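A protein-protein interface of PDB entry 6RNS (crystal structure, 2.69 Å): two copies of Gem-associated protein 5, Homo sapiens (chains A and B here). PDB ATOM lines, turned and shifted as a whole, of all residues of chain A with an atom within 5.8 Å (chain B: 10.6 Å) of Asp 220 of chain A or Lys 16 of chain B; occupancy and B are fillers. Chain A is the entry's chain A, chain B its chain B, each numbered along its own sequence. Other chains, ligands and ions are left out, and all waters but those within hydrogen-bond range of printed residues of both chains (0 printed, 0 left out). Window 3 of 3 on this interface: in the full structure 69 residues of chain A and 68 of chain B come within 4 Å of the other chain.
Hydrophobic or aromatic side chains of chain A that line the printed part of chain B: Ala 196.
Among the printed residues, 6 pairs touch across the chains.
No position is printed for both chains.
Of the 6 pairs that touch across the chains among the printed residues, none has its exchanged pair printed and touching as well.
Of chain B, only Lys 16 comes within 4 Å of Lys 218 of chain A.
Asp 220 of chain A touches one residue of chain B.
Ala 221 of chain A touches none of the printed residues of chain B.
No residue of chain B comes within 4 Å of Ala 222 of chain A.
Ser 223 of chain A touches just these residues of chain B: Lys 16 and His 20.
No residue of chain B comes within 4 Å of Leu 224 of chain A.
Ser 10 of chain B touches none of the printed residues of chain A.
Lys 16 of chain B touches just these residues of chain A: Lys 218 (3.0 Å), Asp 220 (2.9 Å) and Ser 223 (3.3 Å).
Of the printed residues of chain A, His 20 of chain B touches Ser 223 (3.7 Å).
Printed residues of chain A within 4 Å of Cys 23 of chain B: Ala 196.
Leu 24 of chain B touches none of the printed residues of chain A.
The side-chain hydroxyl (OG) of Ser 223 of chain A lies within hydrogen-bond range of the side-chain amino group (NZ) of Lys 16 of chain B, at 3.3 Å.
OD1 of Asp 220 of chain A is in salt-bridge range of NZ of Lys 16 of chain B (2.9 Å).
The side-chain sulfur (SG) of Cys 23 of chain B sits at hydrogen-bond distance from the backbone carbonyl oxygen (O) of Ala 196 of chain A, 3.7 Å away.
Among the printed residues, merely in contact across the chains: Ala 196 of chain A with Leu 19 of chain B (3.7 Å), Lys 218 of chain A with Lys 16 of chain B (3.0 Å) and Ser 223 of chain A with His 20 of chain B (3.7 Å).
The side-chain carboxylate (OD1) of Asp 220 of chain A lies close to the backbone NH (N) of Ser 223 of chain A, 3.2 Å away.
ND1 of His 20 of chain B sits close to O of Lys 16 of chain B (3.5 Å).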
ATOM      1  N   ALA A 196     -21.440  -6.277  -8.069  1.00  0.00           N
ATOM      2  CA  ALA A 196     -20.605  -7.308  -8.678  1.00  0.00           C
ATOM      3  C   ALA A 196     -19.387  -7.607  -7.811  1.00  0.00           C
ATOM      4  O   ALA A 196     -19.050  -8.773  -7.578  1.00  0.00           O
ATOM      5  CB  ALA A 196     -20.178  -6.877 -10.082  1.00  0.00           C
ATOM      6  N   ALA A 216     -27.819 -10.581  -7.812  1.00  0.00           N
ATOM      7  CA  ALA A 216     -29.153 -10.365  -8.358  1.00  0.00           C
ATOM      8  C   ALA A 216     -29.750  -9.040  -7.898  1.00  0.00           C
ATOM      9  O   ALA A 216     -30.615  -8.486  -8.586  1.00  0.00           O
ATOM     10  CB  ALA A 216     -30.078 -11.516  -7.958  1.00  0.00           C
ATOM     11  N   LYS A 218     -28.678  -6.215  -8.155  1.00  0.00           N
ATOM     12  CA  LYS A 218     -28.527  -5.231  -9.223  1.00  0.00           C
ATOM     13  C   LYS A 218     -29.825  -5.093 -10.010  1.00  0.00           C
ATOM     14  O   LYS A 218     -30.364  -3.990 -10.157  1.00  0.00           O
ATOM     15  CB  LYS A 218     -27.367  -5.631 -10.135  1.00  0.00           C
ATOM     16  CG  LYS A 218     -27.085  -4.654 -11.268  1.00  0.00           C
ATOM     17  CD  LYS A 218     -26.909  -3.229 -10.766  1.00  0.00           C
ATOM     18  CE  LYS A 218     -26.362  -2.323 -11.860  1.00  0.00           C
ATOM     19  NZ  LYS A 218     -26.334  -0.893 -11.446  1.00  0.00           N
ATOM     20  N   GLY A 219     -30.344  -6.210 -10.525  1.00  0.00           N
ATOM     21  CA  GLY A 219     -31.685  -6.270 -11.056  1.00  0.00           C
ATOM     22  C   GLY A 219     -31.793  -6.292 -12.565  1.00  0.00           C
ATOM     23  O   GLY A 219     -32.844  -6.678 -13.087  1.00  0.00           O
ATOM     24  N   ASP A 220     -30.751  -5.885 -13.282  1.00  0.00           N
ATOM     25  CA  ASP A 220     -30.847  -5.827 -14.731  1.00  0.00           C
ATOM     26  C   ASP A 220     -30.764  -7.231 -15.330  1.00  0.00           C
ATOM     27  O   ASP A 220     -30.539  -8.227 -14.636  1.00  0.00           O
ATOM     28  CB  ASP A 220     -29.756  -4.930 -15.314  1.00  0.00           C
ATOM     29  CG  ASP A 220     -28.366  -5.496 -15.121  1.00  0.00           C
ATOM     30  OD1 ASP A 220     -28.074  -5.997 -14.016  1.00  0.00           O
ATOM     31  OD2 ASP A 220     -27.563  -5.438 -16.076  1.00  0.00           O
ATOM     32  N   ALA A 221     -30.952  -7.299 -16.650  1.00  0.00           N
ATOM     33  CA  ALA A 221     -31.005  -8.586 -17.332  1.00  0.00           C
ATOM     34  C   ALA A 221     -29.670  -9.318 -17.279  1.00  0.00           C
ATOM     35  O   ALA A 221     -29.646 -10.553 -17.226  1.00  0.00           O
ATOM     36  CB  ALA A 221     -31.437  -8.387 -18.785  1.00  0.00           C
ATOM     37  N   ALA A 222     -28.556  -8.584 -17.303  1.00  0.00           N
ATOM     38  CA  ALA A 222     -27.246  -9.227 -17.294  1.00  0.00           C
ATOM     39  C   ALA A 222     -26.879  -9.730 -15.903  1.00  0.00           C
ATOM     40  O   ALA A 222     -26.258 -10.790 -15.771  1.00  0.00           O
ATOM     41  CB  ALA A 222     -26.184  -8.255 -17.807  1.00  0.00           C
ATOM     42  N   SER A 223     -27.255  -8.987 -14.859  1.00  0.00           N
ATOM     43  CA  SER A 223     -26.936  -9.402 -13.497  1.00  0.00           C
ATOM     44  C   SER A 223     -27.659 -10.692 -13.132  1.00  0.00           C
ATOM     45  O   SER A 223     -27.035 -11.653 -12.666  1.00  0.00           O
ATOM     46  CB  SER A 223     -27.306  -8.293 -12.510  1.00  0.00           C
ATOM     47  OG  SER A 223     -26.493  -7.148 -12.689  1.00  0.00           O
ATOM     48  N   LEU A 224     -28.981 -10.723 -13.321  1.00  0.00           N
ATOM     49  CA  LEU A 224     -29.747 -11.927 -13.023  1.00  0.00           C
ATOM     50  C   LEU A 224     -29.241 -13.110 -13.836  1.00  0.00           C
ATOM     51  O   LEU A 224     -29.152 -14.233 -13.324  1.00  0.00           O
ATOM     52  CB  LEU A 224     -31.228 -11.676 -13.297  1.00  0.00           C
ATOM     53  CG  LEU A 224     -31.910 -10.661 -12.379  1.00  0.00           C
ATOM     54  CD1 LEU A 224     -33.168 -10.104 -13.026  1.00  0.00           C
ATOM     55  CD2 LEU A 224     -32.233 -11.297 -11.032  1.00  0.00           C
ATOM     56  N   ARG A 225     -28.896 -12.875 -15.105  1.00  0.00           N
ATOM     57  CA  ARG A 225     -28.366 -13.940 -15.949  1.00  0.00           C
ATOM     58  C   ARG A 225     -27.107 -14.545 -15.341  1.00  0.00           C
ATOM     59  O   ARG A 225     -27.021 -15.764 -15.148  1.00  0.00           O
ATOM     60  CB  ARG A 225     -28.080 -13.393 -17.347  1.00  0.00           C
ATOM     61  CG  ARG A 225     -27.398 -14.375 -18.285  1.00  0.00           C
ATOM     62  CD  ARG A 225     -28.233 -15.628 -18.489  1.00  0.00           C
ATOM     63  NE  ARG A 225     -27.825 -16.348 -19.691  1.00  0.00           N
ATOM     64  CZ  ARG A 225     -28.293 -16.095 -20.911  1.00  0.00           C
ATOM     65  NH1 ARG A 225     -29.191 -15.136 -21.099  1.00  0.00           N
ATOM     66  NH2 ARG A 225     -27.859 -16.803 -21.945  1.00  0.00           N
ATOM     67  N   GLU A 250     -37.502  -9.618 -16.761  1.00  0.00           N
ATOM     68  CA  GLU A 250     -36.895  -8.371 -17.215  1.00  0.00           C
ATOM     69  C   GLU A 250     -36.923  -8.263 -18.734  1.00  0.00           C
ATOM     70  O   GLU A 250     -36.996  -7.154 -19.277  1.00  0.00           O
ATOM     71  CB  GLU A 250     -35.459  -8.273 -16.700  1.00  0.00           C
ATOM     72  CG  GLU A 250     -34.905  -6.857 -16.651  1.00  0.00           C
ATOM     73  CD  GLU A 250     -35.618  -5.989 -15.632  1.00  0.00           C
ATOM     74  OE1 GLU A 250     -36.450  -6.526 -14.868  1.00  0.00           O
ATOM     75  OE2 GLU A 250     -35.349  -4.770 -15.595  1.00  0.00           O
ATOM     76  N   SER B  10      -6.770  -1.703 -10.777  1.00  0.00           N
ATOM     77  CA  SER B  10      -7.343  -1.261 -12.043  1.00  0.00           C
ATOM     78  C   SER B  10      -8.267  -2.321 -12.629  1.00  0.00           C
ATOM     79  O   SER B  10      -9.366  -1.998 -13.099  1.00  0.00           O
ATOM     80  CB  SER B  10      -6.224  -0.924 -13.029  1.00  0.00           C
ATOM     81  OG  SER B  10      -6.746  -0.421 -14.245  1.00  0.00           O
ATOM     82  N   LEU B  11      -7.848  -3.587 -12.602  1.00  0.00           N
ATOM     83  CA  LEU B  11      -8.663  -4.653 -13.166  1.00  0.00           C
ATOM     84  C   LEU B  11      -9.909  -4.935 -12.336  1.00  0.00           C
ATOM     85  O   LEU B  11     -10.842  -5.570 -12.842  1.00  0.00           O
ATOM     86  CB  LEU B  11      -7.837  -5.932 -13.300  1.00  0.00           C
ATOM     87  CG  LEU B  11      -6.528  -5.833 -14.084  1.00  0.00           C
ATOM     88  CD1 LEU B  11      -6.116  -7.212 -14.602  1.00  0.00           C
ATOM     89  CD2 LEU B  11      -6.626  -4.833 -15.224  1.00  0.00           C
ATOM     90  N   ASP B  12      -9.942  -4.500 -11.075  1.00  0.00           N
ATOM     91  CA  ASP B  12     -11.151  -4.595 -10.268  1.00  0.00           C
ATOM     92  C   ASP B  12     -12.085  -3.408 -10.469  1.00  0.00           C
ATOM     93  O   ASP B  12     -13.283  -3.521 -10.183  1.00  0.00           O
ATOM     94  CB  ASP B  12     -10.799  -4.700  -8.779  1.00  0.00           C
ATOM     95  CG  ASP B  12     -10.596  -6.133  -8.323  1.00  0.00           C
ATOM     96  OD1 ASP B  12     -10.389  -7.016  -9.183  1.00  0.00           O
ATOM     97  OD2 ASP B  12     -10.657  -6.377  -7.096  1.00  0.00           O
ATOM     98  N   HIS B  13     -11.561  -2.276 -10.941  1.00  0.00           N
ATOM     99  CA  HIS B  13     -12.380  -1.106 -11.229  1.00  0.00           C
ATOM    100  C   HIS B  13     -12.521  -0.919 -12.734  1.00  0.00           C
ATOM    101  O   HIS B  13     -12.066   0.085 -13.290  1.00  0.00           O
ATOM    102  CB  HIS B  13     -11.778   0.147 -10.593  1.00  0.00           C
ATOM    103  CG  HIS B  13     -11.957   0.216  -9.109  1.00  0.00           C
ATOM    104  ND1 HIS B  13     -11.059  -0.342  -8.224  1.00  0.00           N
ATOM    105  CD2 HIS B  13     -12.934   0.771  -8.354  1.00  0.00           C
ATOM    106  CE1 HIS B  13     -11.473  -0.128  -6.988  1.00  0.00           C
ATOM    107  NE2 HIS B  13     -12.609   0.543  -7.038  1.00  0.00           N
ATOM    108  N   ARG B  14     -13.132  -1.895 -13.398  1.00  0.00           N
ATOM    109  CA  ARG B  14     -13.405  -1.798 -14.824  1.00  0.00           C
ATOM    110  C   ARG B  14     -14.849  -2.216 -15.086  1.00  0.00           C
ATOM    111  O   ARG B  14     -15.649  -2.297 -14.139  1.00  0.00           O
ATOM    112  CB  ARG B  14     -12.406  -2.644 -15.621  1.00  0.00           C
ATOM    113  CG  ARG B  14     -12.218  -4.075 -15.158  1.00  0.00           C
ATOM    114  CD  ARG B  14     -11.269  -4.822 -16.093  1.00  0.00           C
ATOM    115  NE  ARG B  14     -11.220  -6.256 -15.817  1.00  0.00           N
ATOM    116  CZ  ARG B  14     -10.550  -7.136 -16.555  1.00  0.00           C
ATOM    117  NH1 ARG B  14     -10.560  -8.422 -16.231  1.00  0.00           N
ATOM    118  NH2 ARG B  14      -9.870  -6.732 -17.619  1.00  0.00           N
ATOM    119  N   SER B  15     -15.193  -2.472 -16.341  1.00  0.00           N
ATOM    120  CA  SER B  15     -16.583  -2.532 -16.761  1.00  0.00           C
ATOM    121  C   SER B  15     -17.372  -3.571 -15.968  1.00  0.00           C
ATOM    122  O   SER B  15     -16.824  -4.521 -15.403  1.00  0.00           O
ATOM    123  CB  SER B  15     -16.666  -2.856 -18.254  1.00  0.00           C
ATOM    124  OG  SER B  15     -16.441  -4.236 -18.494  1.00  0.00           O
ATOM    125  N   LYS B  16     -18.693  -3.366 -15.930  1.00  0.00           N
ATOM    126  CA  LYS B  16     -19.589  -4.342 -15.322  1.00  0.00           C
ATOM    127  C   LYS B  16     -19.618  -5.639 -16.118  1.00  0.00           C
ATOM    128  O   LYS B  16     -19.755  -6.719 -15.529  1.00  0.00           O
ATOM    129  CB  LYS B  16     -20.991  -3.742 -15.211  1.00  0.00           C
ATOM    130  CG  LYS B  16     -22.027  -4.646 -14.577  1.00  0.00           C
ATOM    131  CD  LYS B  16     -23.404  -4.005 -14.656  1.00  0.00           C
ATOM    132  CE  LYS B  16     -24.469  -4.885 -14.032  1.00  0.00           C
ATOM    133  NZ  LYS B  16     -25.812  -4.259 -14.149  1.00  0.00           N
ATOM    134  N   GLU B  17     -19.488  -5.555 -17.443  1.00  0.00           N
ATOM    135  CA  GLU B  17     -19.346  -6.759 -18.250  1.00  0.00           C
ATOM    136  C   GLU B  17     -18.132  -7.563 -17.800  1.00  0.00           C
ATOM    137  O   GLU B  17     -18.212  -8.782 -17.605  1.00  0.00           O
ATOM    138  CB  GLU B  17     -19.215  -6.390 -19.728  1.00  0.00           C
ATOM    139  CG  GLU B  17     -20.203  -5.347 -20.226  1.00  0.00           C
ATOM    140  CD  GLU B  17     -19.982  -4.995 -21.689  1.00  0.00           C
ATOM    141  OE1 GLU B  17     -19.386  -3.934 -21.968  1.00  0.00           O
ATOM    142  OE2 GLU B  17     -20.396  -5.791 -22.560  1.00  0.00           O
ATOM    143  N   GLU B  18     -16.992  -6.886 -17.629  1.00  0.00           N
ATOM    144  CA  GLU B  18     -15.776  -7.555 -17.179  1.00  0.00           C
ATOM    145  C   GLU B  18     -15.944  -8.125 -15.776  1.00  0.00           C
ATOM    146  O   GLU B  18     -15.456  -9.222 -15.480  1.00  0.00           O
ATOM    147  CB  GLU B  18     -14.601  -6.577 -17.217  1.00  0.00           C
ATOM    148  CG  GLU B  18     -13.936  -6.437 -18.576  1.00  0.00           C
ATOM    149  CD  GLU B  18     -13.260  -7.719 -19.020  1.00  0.00           C
ATOM    150  OE1 GLU B  18     -12.741  -7.758 -20.155  1.00  0.00           O
ATOM    151  OE2 GLU B  18     -13.251  -8.689 -18.233  1.00  0.00           O
ATOM    152  N   LEU B  19     -16.628  -7.391 -14.894  1.00  0.00           N
ATOM    153  CA  LEU B  19     -16.818  -7.863 -13.527  1.00  0.00           C
ATOM    154  C   LEU B  19     -17.604  -9.168 -13.495  1.00  0.00           C
ATOM    155  O   LEU B  19     -17.298 -10.064 -12.700  1.00  0.00           O
ATOM    156  CB  LEU B  19     -17.531  -6.793 -12.701  1.00  0.00           C
ATOM    157  CG  LEU B  19     -16.639  -5.887 -11.853  1.00  0.00           C
ATOM    158  CD1 LEU B  19     -17.427  -4.714 -11.290  1.00  0.00           C
ATOM    159  CD2 LEU B  19     -15.994  -6.693 -10.729  1.00  0.00           C
ATOM    160  N   HIS B  20     -18.627  -9.292 -14.347  1.00  0.00           N
ATOM    161  CA  HIS B  20     -19.467 -10.483 -14.324  1.00  0.00           C
ATOM    162  C   HIS B  20     -18.709 -11.720 -14.784  1.00  0.00           C
ATOM    163  O   HIS B  20     -18.955 -12.817 -14.267  1.00  0.00           O
ATOM    164  CB  HIS B  20     -20.706 -10.256 -15.192  1.00  0.00           C
ATOM    165  CG  HIS B  20     -21.723  -9.351 -14.566  1.00  0.00           C
ATOM    166  ND1 HIS B  20     -22.655  -8.653 -15.304  1.00  0.00           N
ATOM    167  CD2 HIS B  20     -21.958  -9.037 -13.271  1.00  0.00           C
ATOM    168  CE1 HIS B  20     -23.417  -7.944 -14.489  1.00  0.00           C
ATOM    169  NE2 HIS B  20     -23.016  -8.160 -13.250  1.00  0.00           N
ATOM    170  N   GLN B  21     -17.790 -11.572 -15.739  1.00  0.00           N
ATOM    171  CA  GLN B  21     -16.962 -12.703 -16.132  1.00  0.00           C
ATOM    172  C   GLN B  21     -16.099 -13.183 -14.975  1.00  0.00           C
ATOM    173  O   GLN B  21     -15.856 -14.390 -14.847  1.00  0.00           O
ATOM    174  CB  GLN B  21     -16.086 -12.315 -17.324  1.00  0.00           C
ATOM    175  CG  GLN B  21     -16.862 -11.973 -18.585  1.00  0.00           C
ATOM    176  CD  GLN B  21     -15.953 -11.636 -19.750  1.00  0.00           C
ATOM    177  OE1 GLN B  21     -14.846 -11.133 -19.563  1.00  0.00           O
ATOM    178  NE2 GLN B  21     -16.414 -11.923 -20.961  1.00  0.00           N
ATOM    179  N   ASP B  22     -15.646 -12.264 -14.120  1.00  0.00           N
ATOM    180  CA  ASP B  22     -14.807 -12.646 -12.991  1.00  0.00           C
ATOM    181  C   ASP B  22     -15.565 -13.533 -12.010  1.00  0.00           C
ATOM    182  O   ASP B  22     -15.004 -14.494 -11.472  1.00  0.00           O
ATOM    183  CB  ASP B  22     -14.285 -11.394 -12.281  1.00  0.00           C
ATOM    184  CG  ASP B  22     -13.261 -10.633 -13.109  1.00  0.00           C
ATOM    185  OD1 ASP B  22     -12.970 -11.061 -14.247  1.00  0.00           O
ATOM    186  OD2 ASP B  22     -12.745  -9.607 -12.617  1.00  0.00           O
ATOM    187  N   CYS B  23     -16.843 -13.226 -11.764  1.00  0.00           N
ATOM    188  CA  CYS B  23     -17.623 -14.014 -10.814  1.00  0.00           C
ATOM    189  C   CYS B  23     -17.766 -15.460 -11.276  1.00  0.00           C
ATOM    190  O   CYS B  23     -17.722 -16.387 -10.457  1.00  0.00           O
ATOM    191  CB  CYS B  23     -19.004 -13.388 -10.620  1.00  0.00           C
ATOM    192  SG  CYS B  23     -19.019 -11.794  -9.780  1.00  0.00           S
ATOM    193  N   LEU B  24     -17.952 -15.674 -12.581  1.00  0.00           N
ATOM    194  CA  LEU B  24     -18.191 -17.023 -13.083  1.00  0.00           C
ATOM    195  C   LEU B  24     -16.910 -17.848 -13.084  1.00  0.00           C
ATOM    196  O   LEU B  24     -16.924 -19.024 -12.700  1.00  0.00           O
ATOM    197  CB  LEU B  24     -18.794 -16.957 -14.486  1.00  0.00           C
ATOM    198  CG  LEU B  24     -20.179 -16.309 -14.558  1.00  0.00           C
ATOM    199  CD1 LEU B  24     -20.569 -16.024 -15.999  1.00  0.00           C
ATOM    200  CD2 LEU B  24     -21.226 -17.187 -13.881  1.00  0.00           C
ATOM    201  N   ARG B  46      -6.886 -14.153 -15.952  1.00  0.00           N
ATOM    202  CA  ARG B  46      -7.379 -13.360 -14.824  1.00  0.00           C
ATOM    203  C   ARG B  46      -6.533 -13.639 -13.581  1.00  0.00           C
ATOM    204  O   ARG B  46      -6.946 -14.300 -12.626  1.00  0.00           O
ATOM    205  CB  ARG B  46      -8.857 -13.650 -14.594  1.00  0.00           C
ATOM    206  CG  ARG B  46      -9.692 -13.440 -15.851  1.00  0.00           C
ATOM    207  CD  ARG B  46     -11.180 -13.328 -15.567  1.00  0.00           C
ATOM    208  NE  ARG B  46     -11.764 -12.197 -16.289  1.00  0.00           N
ATOM    209  CZ  ARG B  46     -11.987 -12.178 -17.601  1.00  0.00           C
ATOM    210  NH1 ARG B  46     -11.675 -13.228 -18.347  1.00  0.00           N
ATOM    211  NH2 ARG B  46     -12.518 -11.104 -18.167  1.00  0.00           N
